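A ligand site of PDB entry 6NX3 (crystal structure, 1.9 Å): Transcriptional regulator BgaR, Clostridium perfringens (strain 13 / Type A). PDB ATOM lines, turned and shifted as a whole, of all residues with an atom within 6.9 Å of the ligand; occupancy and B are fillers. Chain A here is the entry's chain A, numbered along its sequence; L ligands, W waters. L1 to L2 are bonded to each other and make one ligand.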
ATOM      1  N   TRP A   5       1.838 -18.661 -29.532  1.00  0.00           N
ATOM      2  CA  TRP A   5       1.759 -17.174 -29.556  1.00  0.00           C
ATOM      3  C   TRP A   5       2.120 -16.707 -30.966  1.00  0.00           C
ATOM      4  O   TRP A   5       3.285 -16.389 -31.207  1.00  0.00           O
ATOM      5  CB  TRP A   5       2.649 -16.495 -28.500  1.00  0.00           C
ATOM      6  CG  TRP A   5       2.258 -15.071 -28.244  1.00  0.00           C
ATOM      7  CD1 TRP A   5       1.348 -14.343 -28.964  1.00  0.00           C
ATOM      8  CD2 TRP A   5       2.728 -14.198 -27.203  1.00  0.00           C
ATOM      9  NE1 TRP A   5       1.202 -13.091 -28.427  1.00  0.00           N
ATOM     10  CE2 TRP A   5       2.067 -12.956 -27.366  1.00  0.00           C
ATOM     11  CE3 TRP A   5       3.679 -14.316 -26.183  1.00  0.00           C
ATOM     12  CZ2 TRP A   5       2.308 -11.862 -26.531  1.00  0.00           C
ATOM     13  CZ3 TRP A   5       3.916 -13.243 -25.360  1.00  0.00           C
ATOM     14  CH2 TRP A   5       3.247 -12.030 -25.535  1.00  0.00           C
ATOM     15  N   GLU A  19      -3.200 -11.532 -33.432  1.00  0.00           N
ATOM     16  CA  GLU A  19      -2.478 -12.672 -32.815  1.00  0.00           C
ATOM     17  C   GLU A  19      -3.484 -13.685 -32.291  1.00  0.00           C
ATOM     18  O   GLU A  19      -4.630 -13.318 -31.985  1.00  0.00           O
ATOM     19  CB  GLU A  19      -1.563 -12.210 -31.677  1.00  0.00           C
ATOM     20  CG  GLU A  19      -2.268 -11.394 -30.621  1.00  0.00           C
ATOM     21  CD  GLU A  19      -1.615 -11.205 -29.240  1.00  0.00           C
ATOM     22  OE1 GLU A  19      -0.594 -11.888 -28.916  1.00  0.00           O
ATOM     23  OE2 GLU A  19      -2.258 -10.564 -28.428  1.00  0.00           O
ATOM     24  N   ILE A  22      -2.254 -19.441 -26.837  1.00  0.00           N
ATOM     25  CA  ILE A  22      -2.663 -20.425 -25.797  1.00  0.00           C
ATOM     26  C   ILE A  22      -1.574 -20.377 -24.741  1.00  0.00           C
ATOM     27  O   ILE A  22      -0.413 -20.458 -25.122  1.00  0.00           O
ATOM     28  CB  ILE A  22      -2.804 -21.851 -26.343  1.00  0.00           C
ATOM     29  CG1 ILE A  22      -3.786 -21.959 -27.517  1.00  0.00           C
ATOM     30  CG2 ILE A  22      -3.191 -22.799 -25.222  1.00  0.00           C
ATOM     31  CD1 ILE A  22      -3.686 -23.260 -28.266  1.00  0.00           C
ATOM     32  N   GLU A  23      -1.945 -20.216 -23.474  1.00  0.00           N
ATOM     33  CA  GLU A  23      -0.968 -20.163 -22.368  1.00  0.00           C
ATOM     34  C   GLU A  23      -1.515 -20.978 -21.201  1.00  0.00           C
ATOM     35  O   GLU A  23      -2.620 -20.698 -20.728  1.00  0.00           O
ATOM     36  CB  GLU A  23      -0.662 -18.727 -21.957  1.00  0.00           C
ATOM     37  CG  GLU A  23       0.417 -18.629 -20.903  1.00  0.00           C
ATOM     38  CD  GLU A  23       1.077 -17.264 -20.705  1.00  0.00           C
ATOM     39  OE1 GLU A  23       1.123 -16.446 -21.671  1.00  0.00           O
ATOM     40  OE2 GLU A  23       1.538 -17.010 -19.557  1.00  0.00           O
ATOM     41  N   GLY A  30       1.494 -14.076 -13.125  1.00  0.00           N
ATOM     42  CA  GLY A  30       0.770 -13.527 -14.288  1.00  0.00           C
ATOM     43  C   GLY A  30       1.391 -12.225 -14.732  1.00  0.00           C
ATOM     44  O   GLY A  30       2.621 -12.141 -14.737  1.00  0.00           O
ATOM     45  N   TYR A  31       0.543 -11.260 -15.077  1.00  0.00           N
ATOM     46  CA  TYR A  31       0.916 -10.069 -15.844  1.00  0.00           C
ATOM     47  C   TYR A  31       0.237  -8.856 -15.237  1.00  0.00           C
ATOM     48  O   TYR A  31      -0.904  -8.977 -14.740  1.00  0.00           O
ATOM     49  CB  TYR A  31       0.617 -10.304 -17.332  1.00  0.00           C
ATOM     50  CG  TYR A  31       1.262 -11.565 -17.853  1.00  0.00           C
ATOM     51  CD1 TYR A  31       2.632 -11.642 -18.069  1.00  0.00           C
ATOM     52  CD2 TYR A  31       0.504 -12.716 -18.022  1.00  0.00           C
ATOM     53  CE1 TYR A  31       3.231 -12.818 -18.474  1.00  0.00           C
ATOM     54  CE2 TYR A  31       1.095 -13.900 -18.436  1.00  0.00           C
ATOM     55  CZ  TYR A  31       2.455 -13.949 -18.656  1.00  0.00           C
ATOM     56  OH  TYR A  31       3.014 -15.126 -19.072  1.00  0.00           O
ATOM     57  N   ASN A  32       0.958  -7.733 -15.208  1.00  0.00           N
ATOM     58  CA  ASN A  32       0.492  -6.455 -14.638  1.00  0.00           C
ATOM     59  C   ASN A  32       1.023  -5.341 -15.558  1.00  0.00           C
ATOM     60  O   ASN A  32       2.226  -5.140 -15.553  1.00  0.00           O
ATOM     61  CB  ASN A  32       0.965  -6.314 -13.184  1.00  0.00           C
ATOM     62  CG  ASN A  32       0.494  -5.031 -12.529  1.00  0.00           C
ATOM     63  OD1 ASN A  32       0.315  -4.004 -13.184  1.00  0.00           O
ATOM     64  ND2 ASN A  32       0.267  -5.061 -11.227  1.00  0.00           N
ATOM     65  N   TYR A  33       0.178  -4.707 -16.358  1.00  0.00           N
ATOM     66  CA  TYR A  33       0.642  -3.753 -17.395  1.00  0.00           C
ATOM     67  C   TYR A  33      -0.530  -2.947 -17.924  1.00  0.00           C
ATOM     68  O   TYR A  33      -1.722  -3.297 -17.711  1.00  0.00           O
ATOM     69  CB  TYR A  33       1.396  -4.494 -18.506  1.00  0.00           C
ATOM     70  CG  TYR A  33       0.546  -5.429 -19.332  1.00  0.00           C
ATOM     71  CD1 TYR A  33       0.306  -6.734 -18.914  1.00  0.00           C
ATOM     72  CD2 TYR A  33      -0.020  -5.024 -20.532  1.00  0.00           C
ATOM     73  CE1 TYR A  33      -0.482  -7.598 -19.664  1.00  0.00           C
ATOM     74  CE2 TYR A  33      -0.788  -5.887 -21.298  1.00  0.00           C
ATOM     75  CZ  TYR A  33      -1.030  -7.168 -20.855  1.00  0.00           C
ATOM     76  OH  TYR A  33      -1.780  -8.030 -21.605  1.00  0.00           O
ATOM     77  N   GLU A  34      -0.188  -1.851 -18.622  1.00  0.00           N
ATOM     78  CA  GLU A  34      -1.143  -1.031 -19.382  1.00  0.00           C
ATOM     79  C   GLU A  34      -1.242  -1.646 -20.780  1.00  0.00           C
ATOM     80  O   GLU A  34      -0.229  -1.779 -21.460  1.00  0.00           O
ATOM     81  CB  GLU A  34      -0.687   0.427 -19.464  1.00  0.00           C
ATOM     82  CG  GLU A  34      -1.656   1.333 -20.232  1.00  0.00           C
ATOM     83  CD  GLU A  34      -1.049   2.727 -20.505  1.00  0.00           C
ATOM     84  OE1 GLU A  34      -0.678   3.368 -19.487  1.00  0.00           O
ATOM     85  OE2 GLU A  34      -0.883   3.168 -21.702  1.00  0.00           O
ATOM     86  N   VAL A  35      -2.457  -1.998 -21.194  1.00  0.00           N
ATOM     87  CA  VAL A  35      -2.673  -2.718 -22.480  1.00  0.00           C
ATOM     88  C   VAL A  35      -2.305  -1.760 -23.637  1.00  0.00           C
ATOM     89  O   VAL A  35      -2.787  -0.611 -23.638  1.00  0.00           O
ATOM     90  CB  VAL A  35      -4.111  -3.248 -22.578  1.00  0.00           C
ATOM     91  CG1 VAL A  35      -4.399  -3.851 -23.956  1.00  0.00           C
ATOM     92  CG2 VAL A  35      -4.412  -4.243 -21.443  1.00  0.00           C
ATOM     93  N   LEU A  36      -1.469  -2.223 -24.560  1.00  0.00           N
ATOM     94  CA  LEU A  36      -1.034  -1.462 -25.767  1.00  0.00           C
ATOM     95  C   LEU A  36      -1.789  -1.957 -27.013  1.00  0.00           C
ATOM     96  O   LEU A  36      -1.997  -1.148 -27.936  1.00  0.00           O
ATOM     97  CB  LEU A  36       0.473  -1.646 -25.927  1.00  0.00           C
ATOM     98  CG  LEU A  36       1.275  -1.155 -24.714  1.00  0.00           C
ATOM     99  CD1 LEU A  36       2.752  -1.425 -24.855  1.00  0.00           C
ATOM    100  CD2 LEU A  36       1.014   0.312 -24.455  1.00  0.00           C
ATOM    101  N   LYS A  37      -2.201  -3.225 -27.045  1.00  0.00           N
ATOM    102  CA  LYS A  37      -2.915  -3.797 -28.217  1.00  0.00           C
ATOM    103  C   LYS A  37      -4.330  -3.247 -28.288  1.00  0.00           C
ATOM    104  O   LYS A  37      -4.849  -2.805 -27.262  1.00  0.00           O
ATOM    105  CB  LYS A  37      -2.824  -5.324 -28.159  1.00  0.00           C
ATOM    106  CG  LYS A  37      -1.443  -5.831 -28.531  1.00  0.00           C
ATOM    107  CD  LYS A  37      -1.002  -7.126 -27.892  1.00  0.00           C
ATOM    108  CE  LYS A  37       0.388  -7.504 -28.345  1.00  0.00           C
ATOM    109  NZ  LYS A  37       0.793  -8.815 -27.792  1.00  0.00           N
ATOM    110  N   VAL A  40      -8.145  -7.738 -27.085  1.00  0.00           N
ATOM    111  CA  VAL A  40      -7.687  -9.134 -26.960  1.00  0.00           C
ATOM    112  C   VAL A  40      -8.701  -9.884 -26.102  1.00  0.00           C
ATOM    113  O   VAL A  40      -8.756  -9.610 -24.861  1.00  0.00           O
ATOM    114  CB  VAL A  40      -6.275  -9.226 -26.357  1.00  0.00           C
ATOM    115  CG1 VAL A  40      -5.765 -10.632 -26.496  1.00  0.00           C
ATOM    116  CG2 VAL A  40      -5.309  -8.228 -26.977  1.00  0.00           C
ATOM    117  N   HIS A  42      -9.857 -13.174 -24.215  1.00  0.00           N
ATOM    118  CA  HIS A  42      -9.306 -14.357 -23.539  1.00  0.00           C
ATOM    119  C   HIS A  42     -10.474 -15.285 -23.150  1.00  0.00           C
ATOM    120  O   HIS A  42     -11.480 -14.784 -22.636  1.00  0.00           O
ATOM    121  CB  HIS A  42      -8.487 -13.977 -22.302  1.00  0.00           C
ATOM    122  CG  HIS A  42      -7.222 -13.247 -22.604  1.00  0.00           C
ATOM    123  ND1 HIS A  42      -7.212 -11.967 -23.101  1.00  0.00           N
ATOM    124  CD2 HIS A  42      -5.923 -13.596 -22.428  1.00  0.00           C
ATOM    125  CE1 HIS A  42      -5.969 -11.575 -23.261  1.00  0.00           C
ATOM    126  NE2 HIS A  42      -5.159 -12.551 -22.834  1.00  0.00           N
ATOM    127  N   PHE A  66     -12.508 -12.746 -20.575  1.00  0.00           N
ATOM    128  CA  PHE A  66     -12.132 -11.371 -20.210  1.00  0.00           C
ATOM    129  C   PHE A  66     -11.543 -10.740 -21.451  1.00  0.00           C
ATOM    130  O   PHE A  66     -10.952 -11.432 -22.265  1.00  0.00           O
ATOM    131  CB  PHE A  66     -11.247 -11.334 -18.957  1.00  0.00           C
ATOM    132  CG  PHE A  66      -9.885 -11.973 -19.049  1.00  0.00           C
ATOM    133  CD1 PHE A  66      -9.716 -13.321 -18.761  1.00  0.00           C
ATOM    134  CD2 PHE A  66      -8.764 -11.222 -19.353  1.00  0.00           C
ATOM    135  CE1 PHE A  66      -8.460 -13.900 -18.767  1.00  0.00           C
ATOM    136  CE2 PHE A  66      -7.512 -11.812 -19.390  1.00  0.00           C
ATOM    137  CZ  PHE A  66      -7.357 -13.152 -19.088  1.00  0.00           C
ATOM    138  N   LEU A  68      -9.179  -7.472 -23.006  1.00  0.00           N
ATOM    139  CA  LEU A  68      -8.203  -6.392 -22.777  1.00  0.00           C
ATOM    140  C   LEU A  68      -8.419  -5.378 -23.892  1.00  0.00           C
ATOM    141  O   LEU A  68      -8.511  -5.787 -25.069  1.00  0.00           O
ATOM    142  CB  LEU A  68      -6.795  -6.975 -22.823  1.00  0.00           C
ATOM    143  CG  LEU A  68      -6.501  -8.137 -21.870  1.00  0.00           C
ATOM    144  CD1 LEU A  68      -5.035  -8.512 -21.906  1.00  0.00           C
ATOM    145  CD2 LEU A  68      -6.913  -7.825 -20.440  1.00  0.00           C
ATOM    146  N   TYR A  76      -3.582  -9.892 -14.315  1.00  0.00           N
ATOM    147  CA  TYR A  76      -4.233 -11.224 -14.356  1.00  0.00           C
ATOM    148  C   TYR A  76      -3.204 -12.275 -14.005  1.00  0.00           C
ATOM    149  O   TYR A  76      -2.087 -12.291 -14.595  1.00  0.00           O
ATOM    150  CB  TYR A  76      -4.970 -11.423 -15.686  1.00  0.00           C
ATOM    151  CG  TYR A  76      -4.227 -11.161 -16.958  1.00  0.00           C
ATOM    152  CD1 TYR A  76      -4.064  -9.871 -17.441  1.00  0.00           C
ATOM    153  CD2 TYR A  76      -3.803 -12.206 -17.760  1.00  0.00           C
ATOM    154  CE1 TYR A  76      -3.416  -9.625 -18.649  1.00  0.00           C
ATOM    155  CE2 TYR A  76      -3.157 -11.980 -18.980  1.00  0.00           C
ATOM    156  CZ  TYR A  76      -2.951 -10.679 -19.421  1.00  0.00           C
ATOM    157  OH  TYR A  76      -2.311 -10.439 -20.607  1.00  0.00           O
ATOM    158  N   TYR A  86      -5.622 -20.436 -20.779  1.00  0.00           N
ATOM    159  CA  TYR A  86      -6.513 -19.561 -21.580  1.00  0.00           C
ATOM    160  C   TYR A  86      -6.018 -19.498 -23.030  1.00  0.00           C
ATOM    161  O   TYR A  86      -4.850 -19.717 -23.335  1.00  0.00           O
ATOM    162  CB  TYR A  86      -6.700 -18.204 -20.906  1.00  0.00           C
ATOM    163  CG  TYR A  86      -5.461 -17.401 -20.601  1.00  0.00           C
ATOM    164  CD1 TYR A  86      -4.607 -16.953 -21.589  1.00  0.00           C
ATOM    165  CD2 TYR A  86      -5.178 -17.002 -19.297  1.00  0.00           C
ATOM    166  CE1 TYR A  86      -3.497 -16.184 -21.295  1.00  0.00           C
ATOM    167  CE2 TYR A  86      -4.077 -16.227 -19.001  1.00  0.00           C
ATOM    168  CZ  TYR A  86      -3.211 -15.843 -19.989  1.00  0.00           C
ATOM    169  OH  TYR A  86      -2.126 -15.070 -19.668  1.00  0.00           O
ATOM    170  N   TRP A  88      -6.461 -16.923 -26.491  1.00  0.00           N
ATOM    171  CA  TRP A  88      -6.756 -15.518 -26.792  1.00  0.00           C
ATOM    172  C   TRP A  88      -6.692 -15.222 -28.280  1.00  0.00           C
ATOM    173  O   TRP A  88      -5.925 -15.870 -28.989  1.00  0.00           O
ATOM    174  CB  TRP A  88      -5.866 -14.572 -26.006  1.00  0.00           C
ATOM    175  CG  TRP A  88      -4.468 -14.420 -26.492  1.00  0.00           C
ATOM    176  CD1 TRP A  88      -3.986 -13.542 -27.418  1.00  0.00           C
ATOM    177  CD2 TRP A  88      -3.325 -15.108 -25.962  1.00  0.00           C
ATOM    178  NE1 TRP A  88      -2.622 -13.658 -27.511  1.00  0.00           N
ATOM    179  CE2 TRP A  88      -2.190 -14.600 -26.621  1.00  0.00           C
ATOM    180  CE3 TRP A  88      -3.177 -16.099 -24.984  1.00  0.00           C
ATOM    181  CZ2 TRP A  88      -0.916 -15.058 -26.336  1.00  0.00           C
ATOM    182  CZ3 TRP A  88      -1.899 -16.559 -24.721  1.00  0.00           C
ATOM    183  CH2 TRP A  88      -0.790 -16.038 -25.371  1.00  0.00           C
ATOM    184  N   GLY A  90      -6.305 -11.692 -30.461  1.00  0.00           N
ATOM    185  CA  GLY A  90      -6.054 -10.248 -30.565  1.00  0.00           C
ATOM    186  C   GLY A  90      -6.543  -9.764 -31.920  1.00  0.00           C
ATOM    187  O   GLY A  90      -6.253 -10.444 -32.916  1.00  0.00           O
HETATM  188  C1  LIG L   1       2.202  -7.078 -24.345  1.00  0.00           C
HETATM  189  C2  LIG L   1       1.264  -8.149 -23.772  1.00  0.00           C
HETATM  190  C3  LIG L   1       2.054  -9.058 -22.855  1.00  0.00           C
HETATM  191  C4  LIG L   1       2.733  -8.195 -21.775  1.00  0.00           C
HETATM  192  C5  LIG L   1       3.544  -9.069 -20.818  1.00  0.00           C
HETATM  193  C6  LIG L   1       2.848  -6.310 -23.206  1.00  0.00           C
HETATM  194  O1  LIG L   1       3.718  -5.315 -23.749  1.00  0.00           O
HETATM  195  O2  LIG L   1       1.414  -6.155 -25.095  1.00  0.00           O
HETATM  196  O3  LIG L   1       0.687  -8.839 -24.868  1.00  0.00           O
HETATM  197  O4  LIG L   1       1.189  -9.984 -22.190  1.00  0.00           O
HETATM  198  O5  LIG L   1       3.585  -7.238 -22.423  1.00  0.00           O
HETATM  199  O6  LIG L   1       3.855  -8.335 -19.628  1.00  0.00           O
HETATM  200  C1  LG2 L   2       0.625 -11.060 -22.919  1.00  0.00           C
HETATM  201  C2  LG2 L   2       0.403 -12.169 -21.932  1.00  0.00           C
HETATM  202  C3  LG2 L   2      -0.273 -13.355 -22.635  1.00  0.00           C
HETATM  203  C4  LG2 L   2      -1.579 -12.876 -23.241  1.00  0.00           C
HETATM  204  C5  LG2 L   2      -1.249 -11.722 -24.188  1.00  0.00           C
HETATM  205  C6  LG2 L   2      -2.458 -11.070 -24.861  1.00  0.00           C
HETATM  206  O1  LG2 L   2       1.657 -12.589 -21.441  1.00  0.00           O
HETATM  207  O2  LG2 L   2      -0.465 -14.436 -21.714  1.00  0.00           O
HETATM  208  O3  LG2 L   2      -2.519 -12.457 -22.233  1.00  0.00           O
HETATM  209  O4  LG2 L   2      -0.653 -10.686 -23.441  1.00  0.00           O
HETATM  210  O5  LG2 L   2      -2.052  -9.930 -25.622  1.00  0.00           O
HETATM  211  O   HOH W   1      -1.076  -5.162 -24.838  1.00  0.00           O
HETATM  212  O   HOH W   2      -2.379  -7.515 -24.279  1.00  0.00           O
HETATM  213  O   HOH W   3       3.739  -7.982 -16.866  1.00  0.00           O
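Water W1 lies within hydrogen-bond range of O2 of LIG L1 (2.7 Å), N of Leu 36 (3.0 Å) and N of Lys 37 (3.1 Å). Water W2 lies within hydrogen-bond range of O5 of LG2 L2 (2.8 Å) and OH of Tyr 33 (2.8 Å). Water W3 bridges an oxygen (O6) of LIG L1 (2.8 Å) and the backbone NH of Asn 32 (3.2 Å).
OE2 of Glu 19 sits at hydrogen-bond distance from O5 of LG2 L2, at 2.9 Å. The side-chain amino group of Lys 37 lies within hydrogen-bond range of an oxygen (O3) of LIG L1. An oxygen (O3) of LG2 L2 is in hydrogen-bond range of the side-chain hydroxyl (OH) of Tyr 76, at 2.6 Å. NE2 of His 42 lies within hydrogen-bond range of O3 of LG2 L2, at 2.7 Å. An oxygen (O4) of LG2 L2 sits at hydrogen-bond distance from the side-chain hydroxyl of Tyr 33, 3.4 Å away. The side-chain carboxylate (OE1) of Glu 23 is in hydrogen-bond range of an oxygen (O2) of LG2 L2. An oxygen (O2) of LG2 L2 sits at hydrogen-bond distance from the side-chain hydroxyl of Tyr 86 (2.7 Å).
ND1 of His 42 is in hydrogen-bond range of O of Val 40, at 3.3 Å. The backbone carbonyl oxygen of Phe 66 sits at hydrogen-bond distance from the backbone NH of His 42, at 2.8 Å. The side-chain carboxylate (OE2) of Glu 23 is in hydrogen-bond range of the side-chain hydroxyl (OH) of Tyr 31 (2.4 Å). The side-chain amino group (NZ) of Lys 37 is in salt-bridge range of the side-chain carboxylate (OE1) of Glu 19 (3.6 Å). The backbone carbonyl oxygen (O) of Glu 19 is in hydrogen-bond range of the backbone NH (N) of Gly 90 (2.8 Å). The backbone NH of Val 40 sits at hydrogen-bond distance from the backbone carbonyl oxygen of Leu 68 (2.8 Å). O of Tyr 31 sits at hydrogen-bond distance from N of Tyr 76. The side-chain hydroxyl (OH) of Tyr 76 lies within hydrogen-bond range of the side-chain hydroxyl (OH) of Tyr 33, 2.7 Å away.
Trp 5 touches the ligand. Tyr 31 touches the ligand. CG1 of Val 40 touches C6 of LG2 L2, 3.7 Å away. NE1 of Trp 88 touches C6 of LG2 L2 (3.7 Å). Hydrophobic or aromatic side chains that line the ligand: Trp 5, Tyr 31, Tyr 33, Val 40, His 42, Tyr 76, Tyr 86 and Trp 88. The nearest printed residue that does not touch the ligand is Leu 36 (4.2 Å).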
